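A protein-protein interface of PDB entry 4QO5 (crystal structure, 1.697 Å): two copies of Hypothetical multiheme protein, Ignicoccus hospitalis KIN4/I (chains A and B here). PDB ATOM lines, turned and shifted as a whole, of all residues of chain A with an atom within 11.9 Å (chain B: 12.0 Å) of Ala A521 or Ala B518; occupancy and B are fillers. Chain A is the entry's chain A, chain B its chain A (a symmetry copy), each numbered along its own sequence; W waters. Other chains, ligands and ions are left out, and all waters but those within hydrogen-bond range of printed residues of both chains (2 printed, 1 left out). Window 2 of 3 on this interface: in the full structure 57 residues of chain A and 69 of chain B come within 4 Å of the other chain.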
ATOM      1  N   LEU A 449     -12.090  -3.066  15.440  1.00  0.00           N
ATOM      2  CA  LEU A 449     -12.776  -3.372  14.190  1.00  0.00           C
ATOM      3  C   LEU A 449     -13.613  -2.173  13.751  1.00  0.00           C
ATOM      4  O   LEU A 449     -13.812  -1.946  12.555  1.00  0.00           O
ATOM      5  CB  LEU A 449     -13.648  -4.624  14.331  1.00  0.00           C
ATOM      6  CG  LEU A 449     -14.532  -5.020  13.145  1.00  0.00           C
ATOM      7  CD1 LEU A 449     -13.708  -5.232  11.878  1.00  0.00           C
ATOM      8  CD2 LEU A 449     -15.322  -6.275  13.487  1.00  0.00           C
ATOM      9  N   THR A 510     -19.222 -13.548  13.497  1.00  0.00           N
ATOM     10  CA  THR A 510     -18.329 -13.966  12.423  1.00  0.00           C
ATOM     11  C   THR A 510     -17.336 -12.859  12.035  1.00  0.00           C
ATOM     12  O   THR A 510     -16.134 -13.113  11.885  1.00  0.00           O
ATOM     13  CB  THR A 510     -19.125 -14.460  11.196  1.00  0.00           C
ATOM     14  OG1 THR A 510     -19.751 -15.711  11.520  1.00  0.00           O
ATOM     15  CG2 THR A 510     -18.208 -14.660  10.013  1.00  0.00           C
ATOM     16  N   LEU A 511     -17.830 -11.630  11.906  1.00  0.00           N
ATOM     17  CA  LEU A 511     -16.956 -10.492  11.617  1.00  0.00           C
ATOM     18  C   LEU A 511     -15.881 -10.304  12.694  1.00  0.00           C
ATOM     19  O   LEU A 511     -14.710 -10.089  12.382  1.00  0.00           O
ATOM     20  CB  LEU A 511     -17.772  -9.212  11.435  1.00  0.00           C
ATOM     21  CG  LEU A 511     -18.565  -9.149  10.126  1.00  0.00           C
ATOM     22  CD1 LEU A 511     -19.474  -7.933  10.102  1.00  0.00           C
ATOM     23  CD2 LEU A 511     -17.620  -9.140   8.936  1.00  0.00           C
ATOM     24  N   LEU A 512     -16.284 -10.401  13.958  1.00  0.00           N
ATOM     25  CA  LEU A 512     -15.337 -10.338  15.067  1.00  0.00           C
ATOM     26  C   LEU A 512     -14.294 -11.452  14.996  1.00  0.00           C
ATOM     27  O   LEU A 512     -13.106 -11.210  15.213  1.00  0.00           O
ATOM     28  CB  LEU A 512     -16.077 -10.384  16.409  1.00  0.00           C
ATOM     29  CG  LEU A 512     -16.879  -9.130  16.758  1.00  0.00           C
ATOM     30  CD1 LEU A 512     -17.751  -9.367  17.992  1.00  0.00           C
ATOM     31  CD2 LEU A 512     -15.931  -7.953  16.982  1.00  0.00           C
ATOM     32  N   ARG A 513     -14.742 -12.668  14.688  1.00  0.00           N
ATOM     33  CA  ARG A 513     -13.840 -13.808  14.520  1.00  0.00           C
ATOM     34  C   ARG A 513     -12.844 -13.627  13.379  1.00  0.00           C
ATOM     35  O   ARG A 513     -11.664 -13.955  13.520  1.00  0.00           O
ATOM     36  CB  ARG A 513     -14.628 -15.089  14.263  1.00  0.00           C
ATOM     37  CG  ARG A 513     -15.111 -15.800  15.500  1.00  0.00           C
ATOM     38  CD  ARG A 513     -15.672 -17.162  15.128  1.00  0.00           C
ATOM     39  NE  ARG A 513     -14.642 -18.070  14.625  1.00  0.00           N
ATOM     40  CZ  ARG A 513     -14.837 -18.961  13.655  1.00  0.00           C
ATOM     41  NH1 ARG A 513     -13.848 -19.749  13.264  1.00  0.00           N
ATOM     42  NH2 ARG A 513     -16.025 -19.061  13.070  1.00  0.00           N
ATOM     43  N   LEU A 514     -13.327 -13.146  12.236  1.00  0.00           N
ATOM     44  CA  LEU A 514     -12.448 -12.888  11.092  1.00  0.00           C
ATOM     45  C   LEU A 514     -11.423 -11.821  11.433  1.00  0.00           C
ATOM     46  O   LEU A 514     -10.249 -11.936  11.080  1.00  0.00           O
ATOM     47  CB  LEU A 514     -13.252 -12.441   9.870  1.00  0.00           C
ATOM     48  CG  LEU A 514     -14.054 -13.526   9.154  1.00  0.00           C
ATOM     49  CD1 LEU A 514     -14.842 -12.930   8.000  1.00  0.00           C
ATOM     50  CD2 LEU A 514     -13.132 -14.631   8.662  1.00  0.00           C
ATOM     51  N   TRP A 515     -11.876 -10.782  12.124  1.00  0.00           N
ATOM     52  CA  TRP A 515     -10.992  -9.700  12.535  1.00  0.00           C
ATOM     53  C   TRP A 515      -9.893 -10.201  13.467  1.00  0.00           C
ATOM     54  O   TRP A 515      -8.720  -9.891  13.273  1.00  0.00           O
ATOM     55  CB  TRP A 515     -11.796  -8.577  13.188  1.00  0.00           C
ATOM     56  CG  TRP A 515     -10.981  -7.392  13.597  1.00  0.00           C
ATOM     57  CD1 TRP A 515     -10.746  -6.960  14.873  1.00  0.00           C
ATOM     58  CD2 TRP A 515     -10.298  -6.475  12.730  1.00  0.00           C
ATOM     59  NE1 TRP A 515      -9.959  -5.832  14.853  1.00  0.00           N
ATOM     60  CE2 TRP A 515      -9.668  -5.515  13.551  1.00  0.00           C
ATOM     61  CE3 TRP A 515     -10.159  -6.371  11.340  1.00  0.00           C
ATOM     62  CZ2 TRP A 515      -8.914  -4.465  13.030  1.00  0.00           C
ATOM     63  CZ3 TRP A 515      -9.405  -5.328  10.825  1.00  0.00           C
ATOM     64  CH2 TRP A 515      -8.791  -4.390  11.670  1.00  0.00           C
ATOM     65  N   GLU A 516     -10.271 -10.989  14.466  1.00  0.00           N
ATOM     66  CA  GLU A 516      -9.291 -11.545  15.396  1.00  0.00           C
ATOM     67  C   GLU A 516      -8.325 -12.511  14.713  1.00  0.00           C
ATOM     68  O   GLU A 516      -7.141 -12.541  15.044  1.00  0.00           O
ATOM     69  CB  GLU A 516      -9.980 -12.222  16.582  1.00  0.00           C
ATOM     70  CG  GLU A 516     -10.529 -11.236  17.603  1.00  0.00           C
ATOM     71  CD  GLU A 516      -9.478 -10.243  18.082  1.00  0.00           C
ATOM     72  OE1 GLU A 516      -8.447 -10.686  18.633  1.00  0.00           O
ATOM     73  OE2 GLU A 516      -9.684  -9.021  17.909  1.00  0.00           O
ATOM     74  N   ALA A 517      -8.831 -13.295  13.764  1.00  0.00           N
ATOM     75  CA  ALA A 517      -7.989 -14.225  13.019  1.00  0.00           C
ATOM     76  C   ALA A 517      -6.965 -13.475  12.172  1.00  0.00           C
ATOM     77  O   ALA A 517      -5.832 -13.926  12.021  1.00  0.00           O
ATOM     78  CB  ALA A 517      -8.834 -15.144  12.148  1.00  0.00           C
ATOM     79  N   ALA A 518      -7.371 -12.328  11.632  1.00  0.00           N
ATOM     80  CA  ALA A 518      -6.480 -11.486  10.836  1.00  0.00           C
ATOM     81  C   ALA A 518      -5.434 -10.762  11.686  1.00  0.00           C
ATOM     82  O   ALA A 518      -4.396 -10.350  11.177  1.00  0.00           O
ATOM     83  CB  ALA A 518      -7.285 -10.478  10.020  1.00  0.00           C
ATOM     84  N   ARG A 519      -5.717 -10.598  12.977  1.00  0.00           N
ATOM     85  CA  ARG A 519      -4.790  -9.934  13.891  1.00  0.00           C
ATOM     86  C   ARG A 519      -3.796 -10.921  14.499  1.00  0.00           C
ATOM     87  O   ARG A 519      -2.584 -10.751  14.372  1.00  0.00           O
ATOM     88  CB  ARG A 519      -5.553  -9.210  15.003  1.00  0.00           C
ATOM     89  N   ALA A 520      -4.316 -11.958  15.149  1.00  0.00           N
ATOM     90  CA  ALA A 520      -3.483 -12.955  15.821  1.00  0.00           C
ATOM     91  C   ALA A 520      -2.679 -13.809  14.843  1.00  0.00           C
ATOM     92  O   ALA A 520      -1.813 -14.584  15.253  1.00  0.00           O
ATOM     93  CB  ALA A 520      -4.334 -13.839  16.722  1.00  0.00           C
ATOM     94  N   ALA A 521      -2.973 -13.669  13.552  1.00  0.00           N
ATOM     95  CA  ALA A 521      -2.212 -14.352  12.512  1.00  0.00           C
ATOM     96  C   ALA A 521      -0.764 -13.872  12.499  1.00  0.00           C
ATOM     97  O   ALA A 521      -0.484 -12.709  12.795  1.00  0.00           O
ATOM     98  CB  ALA A 521      -2.855 -14.132  11.151  1.00  0.00           C
ATOM     99  N   SER B 447     -12.367 -26.650   7.312  1.00  0.00           N
ATOM    100  CA  SER B 447     -11.315 -25.659   7.515  1.00  0.00           C
ATOM    101  C   SER B 447     -11.403 -24.999   8.885  1.00  0.00           C
ATOM    102  O   SER B 447     -10.505 -24.259   9.284  1.00  0.00           O
ATOM    103  CB  SER B 447     -11.363 -24.589   6.421  1.00  0.00           C
ATOM    104  OG  SER B 447     -12.434 -23.686   6.636  1.00  0.00           O
ATOM    105  N   GLY B 448     -12.491 -25.259   9.595  1.00  0.00           N
ATOM    106  CA  GLY B 448     -12.657 -24.730  10.936  1.00  0.00           C
ATOM    107  C   GLY B 448     -13.318 -23.363  10.988  1.00  0.00           C
ATOM    108  O   GLY B 448     -13.363 -22.737  12.039  1.00  0.00           O
ATOM    109  N   LEU B 449     -13.833 -22.891   9.859  1.00  0.00           N
ATOM    110  CA  LEU B 449     -14.561 -21.628   9.851  1.00  0.00           C
ATOM    111  C   LEU B 449     -15.875 -21.783  10.612  1.00  0.00           C
ATOM    112  O   LEU B 449     -16.369 -20.828  11.217  1.00  0.00           O
ATOM    113  CB  LEU B 449     -14.816 -21.148   8.417  1.00  0.00           C
ATOM    114  CG  LEU B 449     -15.673 -19.894   8.224  1.00  0.00           C
ATOM    115  CD1 LEU B 449     -15.089 -18.694   8.964  1.00  0.00           C
ATOM    116  CD2 LEU B 449     -15.815 -19.591   6.739  1.00  0.00           C
ATOM    117  N   LYS B 509     -18.144 -18.316  -0.825  1.00  0.00           N
ATOM    118  CA  LYS B 509     -16.778 -18.434  -1.321  1.00  0.00           C
ATOM    119  C   LYS B 509     -15.870 -17.322  -0.794  1.00  0.00           C
ATOM    120  O   LYS B 509     -14.709 -17.562  -0.458  1.00  0.00           O
ATOM    121  CB  LYS B 509     -16.761 -18.481  -2.853  1.00  0.00           C
ATOM    122  CG  LYS B 509     -17.231 -19.817  -3.400  1.00  0.00           C
ATOM    123  CD  LYS B 509     -17.593 -19.747  -4.877  1.00  0.00           C
ATOM    124  CE  LYS B 509     -16.403 -19.414  -5.736  1.00  0.00           C
ATOM    125  NZ  LYS B 509     -16.748 -19.578  -7.184  1.00  0.00           N
ATOM    126  N   THR B 510     -16.401 -16.107  -0.719  1.00  0.00           N
ATOM    127  CA  THR B 510     -15.635 -14.983  -0.193  1.00  0.00           C
ATOM    128  C   THR B 510     -15.262 -15.180   1.284  1.00  0.00           C
ATOM    129  O   THR B 510     -14.110 -14.957   1.680  1.00  0.00           O
ATOM    130  CB  THR B 510     -16.384 -13.649  -0.407  1.00  0.00           C
ATOM    131  OG1 THR B 510     -16.383 -13.336  -1.810  1.00  0.00           O
ATOM    132  CG2 THR B 510     -15.704 -12.531   0.347  1.00  0.00           C
ATOM    133  N   LEU B 511     -16.221 -15.631   2.090  1.00  0.00           N
ATOM    134  CA  LEU B 511     -15.947 -15.927   3.497  1.00  0.00           C
ATOM    135  C   LEU B 511     -14.854 -16.992   3.657  1.00  0.00           C
ATOM    136  O   LEU B 511     -13.949 -16.843   4.478  1.00  0.00           O
ATOM    137  CB  LEU B 511     -17.225 -16.347   4.223  1.00  0.00           C
ATOM    138  CG  LEU B 511     -18.208 -15.202   4.484  1.00  0.00           C
ATOM    139  CD1 LEU B 511     -19.514 -15.730   5.050  1.00  0.00           C
ATOM    140  CD2 LEU B 511     -17.589 -14.177   5.418  1.00  0.00           C
ATOM    141  N   LEU B 512     -14.939 -18.054   2.861  1.00  0.00           N
ATOM    142  CA  LEU B 512     -13.906 -19.084   2.854  1.00  0.00           C
ATOM    143  C   LEU B 512     -12.537 -18.524   2.467  1.00  0.00           C
ATOM    144  O   LEU B 512     -11.528 -18.857   3.090  1.00  0.00           O
ATOM    145  CB  LEU B 512     -14.297 -20.232   1.915  1.00  0.00           C
ATOM    146  CG  LEU B 512     -15.452 -21.108   2.399  1.00  0.00           C
ATOM    147  CD1 LEU B 512     -15.907 -22.069   1.298  1.00  0.00           C
ATOM    148  CD2 LEU B 512     -15.030 -21.879   3.649  1.00  0.00           C
ATOM    149  N   ARG B 513     -12.510 -17.674   1.443  1.00  0.00           N
ATOM    150  CA  ARG B 513     -11.277 -17.013   1.015  1.00  0.00           C
ATOM    151  C   ARG B 513     -10.672 -16.112   2.087  1.00  0.00           C
ATOM    152  O   ARG B 513      -9.456 -16.110   2.290  1.00  0.00           O
ATOM    153  CB  ARG B 513     -11.520 -16.167  -0.233  1.00  0.00           C
ATOM    154  CG  ARG B 513     -11.435 -16.917  -1.536  1.00  0.00           C
ATOM    155  CD  ARG B 513     -11.463 -15.938  -2.698  1.00  0.00           C
ATOM    156  NE  ARG B 513     -10.271 -15.092  -2.743  1.00  0.00           N
ATOM    157  CZ  ARG B 513     -10.273 -13.814  -3.115  1.00  0.00           C
ATOM    158  NH1 ARG B 513      -9.144 -13.121  -3.131  1.00  0.00           N
ATOM    159  NH2 ARG B 513     -11.409 -13.223  -3.467  1.00  0.00           N
ATOM    160  N   LEU B 514     -11.513 -15.316   2.743  1.00  0.00           N
ATOM    161  CA  LEU B 514     -11.044 -14.447   3.825  1.00  0.00           C
ATOM    162  C   LEU B 514     -10.487 -15.270   4.972  1.00  0.00           C
ATOM    163  O   LEU B 514      -9.454 -14.931   5.552  1.00  0.00           O
ATOM    164  CB  LEU B 514     -12.174 -13.557   4.346  1.00  0.00           C
ATOM    165  CG  LEU B 514     -12.594 -12.399   3.444  1.00  0.00           C
ATOM    166  CD1 LEU B 514     -13.757 -11.639   4.061  1.00  0.00           C
ATOM    167  CD2 LEU B 514     -11.418 -11.468   3.192  1.00  0.00           C
ATOM    168  N   TRP B 515     -11.179 -16.357   5.295  1.00  0.00           N
ATOM    169  CA  TRP B 515     -10.741 -17.247   6.362  1.00  0.00           C
ATOM    170  C   TRP B 515      -9.380 -17.859   6.053  1.00  0.00           C
ATOM    171  O   TRP B 515      -8.488 -17.861   6.898  1.00  0.00           O
ATOM    172  CB  TRP B 515     -11.789 -18.330   6.612  1.00  0.00           C
ATOM    173  CG  TRP B 515     -11.455 -19.264   7.730  1.00  0.00           C
ATOM    174  CD1 TRP B 515     -11.176 -20.600   7.627  1.00  0.00           C
ATOM    175  CD2 TRP B 515     -11.372 -18.943   9.126  1.00  0.00           C
ATOM    176  NE1 TRP B 515     -10.925 -21.127   8.872  1.00  0.00           N
ATOM    177  CE2 TRP B 515     -11.037 -20.132   9.809  1.00  0.00           C
ATOM    178  CE3 TRP B 515     -11.552 -17.767   9.865  1.00  0.00           C
ATOM    179  CZ2 TRP B 515     -10.879 -20.180  11.192  1.00  0.00           C
ATOM    180  CZ3 TRP B 515     -11.390 -17.817  11.241  1.00  0.00           C
ATOM    181  CH2 TRP B 515     -11.056 -19.018  11.889  1.00  0.00           C
ATOM    182  N   GLU B 516      -9.215 -18.365   4.836  1.00  0.00           N
ATOM    183  CA  GLU B 516      -7.938 -18.949   4.432  1.00  0.00           C
ATOM    184  C   GLU B 516      -6.814 -17.915   4.390  1.00  0.00           C
ATOM    185  O   GLU B 516      -5.678 -18.221   4.748  1.00  0.00           O
ATOM    186  CB  GLU B 516      -8.061 -19.664   3.086  1.00  0.00           C
ATOM    187  CG  GLU B 516      -8.755 -21.015   3.183  1.00  0.00           C
ATOM    188  CD  GLU B 516      -8.120 -21.928   4.224  1.00  0.00           C
ATOM    189  OE1 GLU B 516      -6.914 -22.230   4.095  1.00  0.00           O
ATOM    190  OE2 GLU B 516      -8.826 -22.342   5.170  1.00  0.00           O
ATOM    191  N   ALA B 517      -7.133 -16.699   3.956  1.00  0.00           N
ATOM    192  CA  ALA B 517      -6.147 -15.625   3.915  1.00  0.00           C
ATOM    193  C   ALA B 517      -5.688 -15.251   5.322  1.00  0.00           C
ATOM    194  O   ALA B 517      -4.520 -14.933   5.532  1.00  0.00           O
ATOM    195  CB  ALA B 517      -6.701 -14.406   3.191  1.00  0.00           C
ATOM    196  N   ALA B 518      -6.613 -15.301   6.278  1.00  0.00           N
ATOM    197  CA  ALA B 518      -6.301 -15.012   7.676  1.00  0.00           C
ATOM    198  C   ALA B 518      -5.493 -16.127   8.344  1.00  0.00           C
ATOM    199  O   ALA B 518      -4.822 -15.893   9.346  1.00  0.00           O
ATOM    200  CB  ALA B 518      -7.580 -14.745   8.466  1.00  0.00           C
ATOM    201  N   ARG B 519      -5.568 -17.336   7.795  1.00  0.00           N
ATOM    202  CA  ARG B 519      -4.830 -18.477   8.336  1.00  0.00           C
ATOM    203  C   ARG B 519      -3.429 -18.574   7.737  1.00  0.00           C
ATOM    204  O   ARG B 519      -2.434 -18.570   8.460  1.00  0.00           O
ATOM    205  CB  ARG B 519      -5.594 -19.780   8.092  1.00  0.00           C
ATOM    206  N   ALA B 520      -3.358 -18.652   6.411  1.00  0.00           N
ATOM    207  CA  ALA B 520      -2.085 -18.797   5.706  1.00  0.00           C
ATOM    208  C   ALA B 520      -1.206 -17.553   5.808  1.00  0.00           C
ATOM    209  O   ALA B 520      -0.042 -17.572   5.403  1.00  0.00           O
ATOM    210  CB  ALA B 520      -2.324 -19.160   4.245  1.00  0.00           C
ATOM    211  N   ALA B 521      -1.770 -16.471   6.341  1.00  0.00           N
ATOM    212  CA  ALA B 521      -1.010 -15.250   6.584  1.00  0.00           C
ATOM    213  C   ALA B 521       0.093 -15.497   7.608  1.00  0.00           C
ATOM    214  O   ALA B 521      -0.065 -16.308   8.522  1.00  0.00           O
ATOM    215  CB  ALA B 521      -1.932 -14.135   7.058  1.00  0.00           C
HETATM  216  O   HOH W   1      -5.158 -16.898  12.544  1.00  0.00           O
HETATM  217  O   HOH W   2     -18.622 -19.914  11.744  1.00  0.00           O
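Of the printed residues of chain A, Ala B518 touches Ala A517, Ala A518 and Ala A521. Leu A514 touches just these residues of chain B: Leu B511 and Trp B515. Ala A517 touches two residues of chain B. No residue of chain B comes within 4 Å of Arg A519. No residue of chain B comes within 4 Å of Ala A520. Trp B515 touches three residues of chain A. No residue of chain A comes within 4 Å of Glu B516. No residue of chain A comes within 4 Å of Ala B520. No residue of chain A comes within 4 Å of Ala B521. Of the printed residues of chain A, Leu B511 touches Leu A514 (3.97 Å). Printed residues of chain B within 4 Å of Ala A518: Ala B518. Of the printed residues of chain A, Gly B448 touches Arg A513 (3.3 Å). Printed residues of chain A within 4 Å of Leu B449: Arg A513. Of the printed residues of chain B, Arg A513 touches Gly B448 (3.3 Å), Leu B449 (2.6 Å) and Trp B515 (3.2 Å). The nearest printed residue of chain A that does not touch Leu B511 is Thr A510 (4.7 Å).
Among the printed residues, merely in contact across the chains: Arg A513 with Trp B515 (3.2 Å), Ala A521 with Ala B518 (3.2 Å), Leu A514 with Trp B515 (3.7 Å), Ala A517 with Trp B515 (3.8 Å), Leu A514 with Leu B511 (3.97 Å) and Ala A518 with Ala B518 (3.99 Å).
O of Leu B449 lies within hydrogen-bond range of NH2 of Arg A513. The backbone carbonyl oxygen (O) of Ala A517 sits close to the backbone carbonyl oxygen (O) of Ala B518 (3.5 Å). The guanidinium group (NH1) of Arg A513 lies within hydrogen-bond range of the backbone carbonyl oxygen (O) of Gly B448.
Water W2 bridges the backbone carbonyl oxygen (O) of Leu B449 (2.5 Å) and the guanidinium group (NH2) of Arg A513 (3.0 Å). Water W1 lies within hydrogen-bond range of O of Ala A517 and O of Ala B518.
Of the 13 printed residues of chain A, 5 touch a printed residue of chain B. Printed residues of chain A that touch a printed residue of chain B: Arg A513, Leu A514, Ala A517, Ala A518 and Ala A521. Hydrophobic or aromatic side chains of chain A that line the printed part of chain B: Leu A514, Ala A517 and Ala A521. Hydrophobic or aromatic side chains of chain B that line the printed part of chain A: Leu B511, Trp B515 and Ala B518. Among the printed residues, no Asp or Glu carboxylate lies within 4 Å of a Lys or Arg side-chain nitrogen of the other chain.
The backbone carbonyl oxygen of Ser B447 lies within hydrogen-bond range of the indole nitrogen of Trp B515, at 3.2 Å.
Arg A513 touches Leu B449, but with the chains exchanged Leu A449 does not touch Arg B513 (14.9 Å). Arg A513 touches Trp B515, but with the chains exchanged Trp A515 does not touch Arg B513 (11.4 Å). Ala A517 touches Ala B518, but with the chains exchanged Ala A518 does not touch Ala B517 (6.6 Å). Ala A518 touches its own counterpart, Ala B518. Positions printed for both chains: 449, 510, 511, 512, 513, 514, 515, 516, 517, 518, 519, 520 and 521.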
